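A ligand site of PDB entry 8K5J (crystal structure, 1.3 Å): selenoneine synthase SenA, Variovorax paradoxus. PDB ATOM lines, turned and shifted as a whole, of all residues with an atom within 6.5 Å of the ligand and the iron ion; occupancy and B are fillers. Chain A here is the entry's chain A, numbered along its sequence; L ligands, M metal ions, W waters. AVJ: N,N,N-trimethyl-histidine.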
ATOM      1  N   TRP A  78      35.785  -3.328 -13.434  1.00  0.00           N
ATOM      2  CA  TRP A  78      34.875  -2.955 -14.507  1.00  0.00           C
ATOM      3  C   TRP A  78      33.826  -4.056 -14.694  1.00  0.00           C
ATOM      4  O   TRP A  78      32.625  -3.764 -14.819  1.00  0.00           O
ATOM      5  CB  TRP A  78      35.622  -2.651 -15.807  1.00  0.00           C
ATOM      6  CG  TRP A  78      34.712  -2.230 -16.905  1.00  0.00           C
ATOM      7  CD1 TRP A  78      34.275  -0.942 -17.103  1.00  0.00           C
ATOM      8  CD2 TRP A  78      33.922  -3.045 -17.787  1.00  0.00           C
ATOM      9  NE1 TRP A  78      33.351  -0.928 -18.111  1.00  0.00           N
ATOM     10  CE2 TRP A  78      33.108  -2.193 -18.553  1.00  0.00           C
ATOM     11  CE3 TRP A  78      33.853  -4.399 -18.026  1.00  0.00           C
ATOM     12  CZ2 TRP A  78      32.197  -2.694 -19.508  1.00  0.00           C
ATOM     13  CZ3 TRP A  78      32.981  -4.900 -18.944  1.00  0.00           C
ATOM     14  CH2 TRP A  78      32.153  -4.048 -19.685  1.00  0.00           C
ATOM     15  N   HIS A  82      29.810  -3.723 -14.558  1.00  0.00           N
ATOM     16  CA  HIS A  82      28.999  -4.100 -15.720  1.00  0.00           C
ATOM     17  C   HIS A  82      27.903  -5.064 -15.330  1.00  0.00           C
ATOM     18  O   HIS A  82      26.778  -4.981 -15.852  1.00  0.00           O
ATOM     19  CB  HIS A  82      29.909  -4.681 -16.811  1.00  0.00           C
ATOM     20  CG  HIS A  82      29.162  -5.272 -17.933  1.00  0.00           C
ATOM     21  ND1 HIS A  82      28.422  -4.553 -18.873  1.00  0.00           N
ATOM     22  CD2 HIS A  82      28.989  -6.567 -18.272  1.00  0.00           C
ATOM     23  CE1 HIS A  82      27.858  -5.457 -19.693  1.00  0.00           C
ATOM     24  NE2 HIS A  82      28.212  -6.653 -19.390  1.00  0.00           N
ATOM     25  N   PHE A  86      24.055  -4.028 -15.941  1.00  0.00           N
ATOM     26  CA  PHE A  86      23.189  -4.802 -16.834  1.00  0.00           C
ATOM     27  C   PHE A  86      21.921  -5.217 -16.116  1.00  0.00           C
ATOM     28  O   PHE A  86      20.800  -5.139 -16.685  1.00  0.00           O
ATOM     29  CB  PHE A  86      23.958  -5.980 -17.392  1.00  0.00           C
ATOM     30  CG  PHE A  86      23.218  -6.778 -18.440  1.00  0.00           C
ATOM     31  CD1 PHE A  86      22.380  -7.812 -18.101  1.00  0.00           C
ATOM     32  CD2 PHE A  86      23.409  -6.539 -19.785  1.00  0.00           C
ATOM     33  CE1 PHE A  86      21.699  -8.561 -19.045  1.00  0.00           C
ATOM     34  CE2 PHE A  86      22.743  -7.310 -20.746  1.00  0.00           C
ATOM     35  CZ  PHE A  86      21.925  -8.333 -20.363  1.00  0.00           C
ATOM     36  N   SER A 123      28.485  -2.102 -22.149  1.00  0.00           N
ATOM     37  CA  SER A 123      29.440  -2.755 -23.045  1.00  0.00           C
ATOM     38  C   SER A 123      29.209  -2.361 -24.472  1.00  0.00           C
ATOM     39  O   SER A 123      30.092  -2.575 -25.297  1.00  0.00           O
ATOM     40  CB  SER A 123      29.505  -4.221 -22.780  1.00  0.00           C
ATOM     41  OG  SER A 123      28.253  -4.810 -22.864  1.00  0.00           O
ATOM     42  N   HIS A 178      23.120 -13.723 -17.835  1.00  0.00           N
ATOM     43  CA  HIS A 178      24.208 -12.790 -18.172  1.00  0.00           C
ATOM     44  C   HIS A 178      25.287 -12.820 -17.095  1.00  0.00           C
ATOM     45  O   HIS A 178      26.486 -12.859 -17.404  1.00  0.00           O
ATOM     46  CB  HIS A 178      23.628 -11.380 -18.323  1.00  0.00           C
ATOM     47  CG  HIS A 178      24.665 -10.343 -18.577  1.00  0.00           C
ATOM     48  ND1 HIS A 178      25.097  -9.451 -17.595  1.00  0.00           N
ATOM     49  CD2 HIS A 178      25.394 -10.073 -19.676  1.00  0.00           C
ATOM     50  CE1 HIS A 178      26.056  -8.648 -18.145  1.00  0.00           C
ATOM     51  NE2 HIS A 178      26.288  -9.063 -19.435  1.00  0.00           N
ATOM     52  N   MET A 181      27.436 -15.868 -17.351  1.00  0.00           N
ATOM     53  CA  MET A 181      28.437 -15.771 -18.426  1.00  0.00           C
ATOM     54  C   MET A 181      29.626 -14.954 -17.979  1.00  0.00           C
ATOM     55  O   MET A 181      30.771 -15.326 -18.293  1.00  0.00           O
ATOM     56  CB  MET A 181      27.806 -15.167 -19.682  1.00  0.00           C
ATOM     57  CG  MET A 181      26.693 -16.007 -20.256  1.00  0.00           C
ATOM     58  SD  MET A 181      26.041 -15.822 -21.813  1.00  0.00           S
ATOM     59  CE  MET A 181      24.419 -15.313 -21.513  1.00  0.00           C
ATOM     60  N   HIS A 182      29.419 -13.854 -17.312  1.00  0.00           N
ATOM     61  CA  HIS A 182      30.570 -13.065 -16.845  1.00  0.00           C
ATOM     62  C   HIS A 182      31.320 -13.780 -15.730  1.00  0.00           C
ATOM     63  O   HIS A 182      32.545 -13.557 -15.620  1.00  0.00           O
ATOM     64  CB  HIS A 182      30.114 -11.651 -16.427  1.00  0.00           C
ATOM     65  CG  HIS A 182      29.907 -10.741 -17.587  1.00  0.00           C
ATOM     66  ND1 HIS A 182      30.934 -10.000 -18.163  1.00  0.00           N
ATOM     67  CD2 HIS A 182      28.822 -10.424 -18.327  1.00  0.00           C
ATOM     68  CE1 HIS A 182      30.466  -9.324 -19.194  1.00  0.00           C
ATOM     69  NE2 HIS A 182      29.156  -9.547 -19.342  1.00  0.00           N
ATOM     70  N   GLU A 184      31.949 -17.070 -15.693  1.00  0.00           N
ATOM     71  CA  GLU A 184      32.860 -17.934 -16.463  1.00  0.00           C
ATOM     72  C   GLU A 184      33.968 -17.079 -17.077  1.00  0.00           C
ATOM     73  O   GLU A 184      35.130 -17.577 -17.074  1.00  0.00           O
ATOM     74  CB  GLU A 184      32.085 -18.682 -17.516  1.00  0.00           C
ATOM     75  CG  GLU A 184      32.995 -19.616 -18.268  1.00  0.00           C
ATOM     76  CD  GLU A 184      32.346 -20.286 -19.423  1.00  0.00           C
ATOM     77  OE1 GLU A 184      32.937 -20.288 -20.535  1.00  0.00           O
ATOM     78  OE2 GLU A 184      31.237 -20.841 -19.268  1.00  0.00           O
ATOM     79  N   ALA A 185      33.696 -15.901 -17.586  1.00  0.00           N
ATOM     80  CA  ALA A 185      34.761 -15.070 -18.151  1.00  0.00           C
ATOM     81  C   ALA A 185      35.780 -14.687 -17.052  1.00  0.00           C
ATOM     82  O   ALA A 185      36.980 -14.659 -17.355  1.00  0.00           O
ATOM     83  CB  ALA A 185      34.139 -13.824 -18.788  1.00  0.00           C
ATOM     84  N   TYR A 188      38.133 -17.709 -16.963  1.00  0.00           N
ATOM     85  CA  TYR A 188      39.117 -17.930 -17.991  1.00  0.00           C
ATOM     86  C   TYR A 188      40.068 -16.737 -18.038  1.00  0.00           C
ATOM     87  O   TYR A 188      41.273 -16.933 -18.340  1.00  0.00           O
ATOM     88  CB  TYR A 188      38.556 -18.270 -19.372  1.00  0.00           C
ATOM     89  CG  TYR A 188      37.664 -17.321 -20.110  1.00  0.00           C
ATOM     90  CD1 TYR A 188      38.187 -16.209 -20.713  1.00  0.00           C
ATOM     91  CD2 TYR A 188      36.312 -17.578 -20.273  1.00  0.00           C
ATOM     92  CE1 TYR A 188      37.406 -15.330 -21.445  1.00  0.00           C
ATOM     93  CE2 TYR A 188      35.515 -16.721 -21.029  1.00  0.00           C
ATOM     94  CZ  TYR A 188      36.068 -15.631 -21.631  1.00  0.00           C
ATOM     95  OH  TYR A 188      35.275 -14.765 -22.378  1.00  0.00           O
ATOM     96  N   TYR A 374      17.928  -7.434 -25.756  1.00  0.00           N
ATOM     97  CA  TYR A 374      19.387  -7.214 -25.752  1.00  0.00           C
ATOM     98  C   TYR A 374      19.894  -7.535 -27.144  1.00  0.00           C
ATOM     99  O   TYR A 374      20.380  -8.629 -27.464  1.00  0.00           O
ATOM    100  CB  TYR A 374      20.066  -8.025 -24.650  1.00  0.00           C
ATOM    101  CG  TYR A 374      21.565  -7.866 -24.621  1.00  0.00           C
ATOM    102  CD1 TYR A 374      22.213  -6.741 -25.068  1.00  0.00           C
ATOM    103  CD2 TYR A 374      22.347  -8.850 -24.072  1.00  0.00           C
ATOM    104  CE1 TYR A 374      23.580  -6.617 -25.038  1.00  0.00           C
ATOM    105  CE2 TYR A 374      23.722  -8.746 -24.046  1.00  0.00           C
ATOM    106  CZ  TYR A 374      24.359  -7.627 -24.514  1.00  0.00           C
ATOM    107  OH  TYR A 374      25.707  -7.478 -24.439  1.00  0.00           O
ATOM    108  N   ASP A 376      22.268  -6.754 -29.103  1.00  0.00           N
ATOM    109  CA  ASP A 376      23.660  -7.014 -29.414  1.00  0.00           C
ATOM    110  C   ASP A 376      24.120  -8.346 -28.887  1.00  0.00           C
ATOM    111  O   ASP A 376      25.313  -8.647 -29.024  1.00  0.00           O
ATOM    112  CB  ASP A 376      24.637  -5.933 -28.888  1.00  0.00           C
ATOM    113  CG  ASP A 376      24.758  -4.645 -29.619  1.00  0.00           C
ATOM    114  OD1 ASP A 376      24.093  -4.582 -30.719  1.00  0.00           O
ATOM    115  OD2 ASP A 376      25.547  -3.658 -29.064  1.00  0.00           O
ATOM    116  N   TYR A 377      23.294  -9.164 -28.272  1.00  0.00           N
ATOM    117  CA  TYR A 377      23.765 -10.464 -27.741  1.00  0.00           C
ATOM    118  C   TYR A 377      24.330 -11.357 -28.829  1.00  0.00           C
ATOM    119  O   TYR A 377      25.416 -11.944 -28.663  1.00  0.00           O
ATOM    120  CB  TYR A 377      22.675 -11.158 -26.942  1.00  0.00           C
ATOM    121  CG  TYR A 377      23.182 -12.468 -26.383  1.00  0.00           C
ATOM    122  CD1 TYR A 377      24.175 -12.539 -25.409  1.00  0.00           C
ATOM    123  CD2 TYR A 377      22.618 -13.668 -26.809  1.00  0.00           C
ATOM    124  CE1 TYR A 377      24.672 -13.751 -24.970  1.00  0.00           C
ATOM    125  CE2 TYR A 377      23.084 -14.884 -26.354  1.00  0.00           C
ATOM    126  CZ  TYR A 377      24.136 -14.925 -25.461  1.00  0.00           C
ATOM    127  OH  TYR A 377      24.650 -16.132 -25.013  1.00  0.00           O
ATOM    128  N   TRP A 381      27.613 -10.766 -34.141  1.00  0.00           N
ATOM    129  CA  TRP A 381      28.677 -11.752 -34.090  1.00  0.00           C
ATOM    130  C   TRP A 381      28.484 -12.839 -35.106  1.00  0.00           C
ATOM    131  O   TRP A 381      29.343 -13.718 -35.275  1.00  0.00           O
ATOM    132  CB  TRP A 381      28.826 -12.319 -32.680  1.00  0.00           C
ATOM    133  CG  TRP A 381      28.648 -11.275 -31.625  1.00  0.00           C
ATOM    134  CD1 TRP A 381      27.587 -11.190 -30.773  1.00  0.00           C
ATOM    135  CD2 TRP A 381      29.385 -10.063 -31.419  1.00  0.00           C
ATOM    136  NE1 TRP A 381      27.642 -10.076 -30.035  1.00  0.00           N
ATOM    137  CE2 TRP A 381      28.697  -9.342 -30.442  1.00  0.00           C
ATOM    138  CE3 TRP A 381      30.541  -9.531 -32.015  1.00  0.00           C
ATOM    139  CZ2 TRP A 381      29.164  -8.122 -29.981  1.00  0.00           C
ATOM    140  CZ3 TRP A 381      30.974  -8.256 -31.583  1.00  0.00           C
ATOM    141  CH2 TRP A 381      30.301  -7.605 -30.556  1.00  0.00           C
ATOM    142  N   TYR A 404      22.117 -24.614 -25.941  1.00  0.00           N
ATOM    143  CA  TYR A 404      22.854 -23.337 -25.898  1.00  0.00           C
ATOM    144  C   TYR A 404      23.910 -23.280 -26.925  1.00  0.00           C
ATOM    145  O   TYR A 404      24.680 -24.240 -27.125  1.00  0.00           O
ATOM    146  CB  TYR A 404      23.449 -23.184 -24.502  1.00  0.00           C
ATOM    147  CG  TYR A 404      24.204 -21.896 -24.304  1.00  0.00           C
ATOM    148  CD1 TYR A 404      23.561 -20.774 -23.861  1.00  0.00           C
ATOM    149  CD2 TYR A 404      25.570 -21.808 -24.533  1.00  0.00           C
ATOM    150  CE1 TYR A 404      24.236 -19.565 -23.690  1.00  0.00           C
ATOM    151  CE2 TYR A 404      26.257 -20.627 -24.370  1.00  0.00           C
ATOM    152  CZ  TYR A 404      25.597 -19.513 -23.912  1.00  0.00           C
ATOM    153  OH  TYR A 404      26.334 -18.355 -23.785  1.00  0.00           O
ATOM    154  N   ARG A 405      24.032 -22.148 -27.620  1.00  0.00           N
ATOM    155  CA  ARG A 405      25.048 -21.946 -28.648  1.00  0.00           C
ATOM    156  C   ARG A 405      26.065 -20.965 -28.122  1.00  0.00           C
ATOM    157  O   ARG A 405      25.743 -19.809 -27.923  1.00  0.00           O
ATOM    158  CB  ARG A 405      24.401 -21.391 -29.912  1.00  0.00           C
ATOM    159  CG  ARG A 405      23.230 -22.234 -30.422  1.00  0.00           C
ATOM    160  CD  ARG A 405      22.530 -21.623 -31.619  1.00  0.00           C
ATOM    161  NE  ARG A 405      23.323 -21.764 -32.834  1.00  0.00           N
ATOM    162  CZ  ARG A 405      23.190 -21.000 -33.902  1.00  0.00           C
ATOM    163  NH1 ARG A 405      22.375 -19.951 -33.882  1.00  0.00           N
ATOM    164  NH2 ARG A 405      23.937 -21.228 -34.987  1.00  0.00           N
ATOM    165  N   ASN A 406      27.304 -21.404 -27.859  1.00  0.00           N
ATOM    166  CA  ASN A 406      28.363 -20.485 -27.574  1.00  0.00           C
ATOM    167  C   ASN A 406      29.011 -20.055 -28.867  1.00  0.00           C
ATOM    168  O   ASN A 406      28.864 -20.744 -29.875  1.00  0.00           O
ATOM    169  CB  ASN A 406      29.365 -21.038 -26.575  1.00  0.00           C
ATOM    170  CG  ASN A 406      29.980 -19.966 -25.723  1.00  0.00           C
ATOM    171  OD1 ASN A 406      29.841 -18.765 -25.950  1.00  0.00           O
ATOM    172  ND2 ASN A 406      30.693 -20.363 -24.685  1.00  0.00           N
ATOM    173  N   PHE A 407      29.760 -18.955 -28.861  1.00  0.00           N
ATOM    174  CA  PHE A 407      30.271 -18.386 -30.103  1.00  0.00           C
ATOM    175  C   PHE A 407      31.486 -17.519 -29.796  1.00  0.00           C
ATOM    176  O   PHE A 407      31.372 -16.546 -29.083  1.00  0.00           O
ATOM    177  CB  PHE A 407      29.161 -17.611 -30.868  1.00  0.00           C
ATOM    178  CG  PHE A 407      28.309 -16.691 -30.043  1.00  0.00           C
ATOM    179  CD1 PHE A 407      27.197 -17.172 -29.359  1.00  0.00           C
ATOM    180  CD2 PHE A 407      28.520 -15.312 -29.992  1.00  0.00           C
ATOM    181  CE1 PHE A 407      26.378 -16.335 -28.658  1.00  0.00           C
ATOM    182  CE2 PHE A 407      27.690 -14.471 -29.250  1.00  0.00           C
ATOM    183  CZ  PHE A 407      26.608 -15.012 -28.613  1.00  0.00           C
ATOM    184  N   PHE A 408      32.604 -17.907 -30.399  1.00  0.00           N
ATOM    185  CA  PHE A 408      33.895 -17.188 -30.281  1.00  0.00           C
ATOM    186  C   PHE A 408      34.551 -17.269 -31.646  1.00  0.00           C
ATOM    187  O   PHE A 408      34.347 -18.205 -32.397  1.00  0.00           O
ATOM    188  CB  PHE A 408      34.772 -17.790 -29.180  1.00  0.00           C
ATOM    189  CG  PHE A 408      34.363 -17.361 -27.786  1.00  0.00           C
ATOM    190  CD1 PHE A 408      34.807 -16.122 -27.313  1.00  0.00           C
ATOM    191  CD2 PHE A 408      33.584 -18.151 -26.992  1.00  0.00           C
ATOM    192  CE1 PHE A 408      34.457 -15.702 -26.023  1.00  0.00           C
ATOM    193  CE2 PHE A 408      33.228 -17.699 -25.730  1.00  0.00           C
ATOM    194  CZ  PHE A 408      33.670 -16.490 -25.258  1.00  0.00           C
HETATM  195  CAA AVJ L   1      30.096 -16.020 -24.020  1.00  0.00           C
HETATM  196  CAB AVJ L   1      30.161 -15.361 -26.348  1.00  0.00           C
HETATM  197  CAC AVJ L   1      28.043 -15.814 -25.296  1.00  0.00           C
HETATM  198  OAH AVJ L   1      30.503 -11.828 -25.277  1.00  0.00           O
HETATM  199  OAL AVJ L   1      31.556 -13.383 -24.210  1.00  0.00           O
HETATM  200  CAM AVJ L   1      28.325 -11.404 -21.827  1.00  0.00           C
HETATM  201  CAP AVJ L   1      28.593 -13.513 -23.284  1.00  0.00           C
HETATM  202  NAR AVJ L   1      27.554 -11.283 -23.867  1.00  0.00           N
HETATM  203  NAT AVJ L   1      27.738 -10.148 -21.970  1.00  0.00           N
HETATM  204  CAX AVJ L   1      30.556 -12.909 -24.738  1.00  0.00           C
HETATM  205  CAY AVJ L   1      28.205 -12.107 -22.965  1.00  0.00           C
HETATM  206  CAZ AVJ L   1      27.287 -10.117 -23.211  1.00  0.00           C
HETATM  207  CBC AVJ L   1      29.259 -13.719 -24.664  1.00  0.00           C
HETATM  208  NBE AVJ L   1      29.396 -15.215 -25.036  1.00  0.00           N
HETATM  209 FE    FE M   1      27.880  -8.473 -20.585  1.00  0.00          FE
HETATM  210  O   HOH W   1      27.316 -11.488 -26.695  1.00  0.00           O
HETATM  211  O   HOH W   2      32.658 -14.243 -22.003  1.00  0.00           O
HETATM  212  O   HOH W   3      29.453  -7.795 -21.812  1.00  0.00           O
HETATM  213  O   HOH W   4      26.549  -7.316 -21.835  1.00  0.00           O
HETATM  214  O   HOH W   5      30.443  -9.332 -23.974  1.00  0.00           O
HETATM  215  O   HOH W   6      33.684 -11.758 -24.453  1.00  0.00           O
HETATM  216  O   HOH W   7      31.356 -18.704 -22.263  1.00  0.00           O
HETATM  217  O   HOH W   8      30.017 -11.879 -28.140  1.00  0.00           O
HETATM  218  O   HOH W   9      31.430 -16.325 -20.909  1.00  0.00           O
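The iron ion is bound by a ring nitrogen (NE2) of His 178, a ring nitrogen (NE2) of His 182, water W3, water W4, a nitrogen (NAT) of the ligand and a ring nitrogen (NE2) of His 82.
Along chain A the residues within 4 Å of the iron ion span positions 82 to 182.
Water W4 lies within hydrogen-bond range of the side-chain hydroxyl (OH) of Tyr 374 and the side-chain hydroxyl (OG) of Ser 123. Water W2 lies within hydrogen-bond range of an oxygen (OAL) of the ligand (2.6 Å) and the side-chain hydroxyl (OH) of Tyr 188 (2.7 Å). Water W1 lies within hydrogen-bond range of O of Tyr 377 (2.8 Å) and NAR of the ligand (2.8 Å). Water W7 bridges the side-chain carboxylate (OE1) of Glu 184 and the side-chain amide nitrogen (ND2) of Asn 406.
The side-chain hydroxyl (OH) of Tyr 377 lies within hydrogen-bond range of the side-chain sulfur (SD) of Met 181, 3.5 Å away. The side-chain sulfur (SD) of Met 181 is in hydrogen-bond range of the side-chain hydroxyl (OH) of Tyr 404, 3.2 Å away. O of Tyr 377 lies close to NE1 of Trp 381 (3.2 Å). The side-chain hydroxyl (OH) of Tyr 404 sits at hydrogen-bond distance from the side-chain hydroxyl (OH) of Tyr 377, 3.0 Å away.
Residues that only touch the ligand: Phe 407, Tyr 374, Asn 406, Tyr 404, Tyr 377, Met 181 and Phe 408. Hydrophobic or aromatic side chains that line the ligand: His 178, Met 181, His 182, Tyr 374, Tyr 377, Phe 407 and Phe 408. Within 4 Å of the ligand: His 178, Met 181, His 182, Tyr 374, Tyr 377, Tyr 404, Asn 406, Phe 407 and Phe 408.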
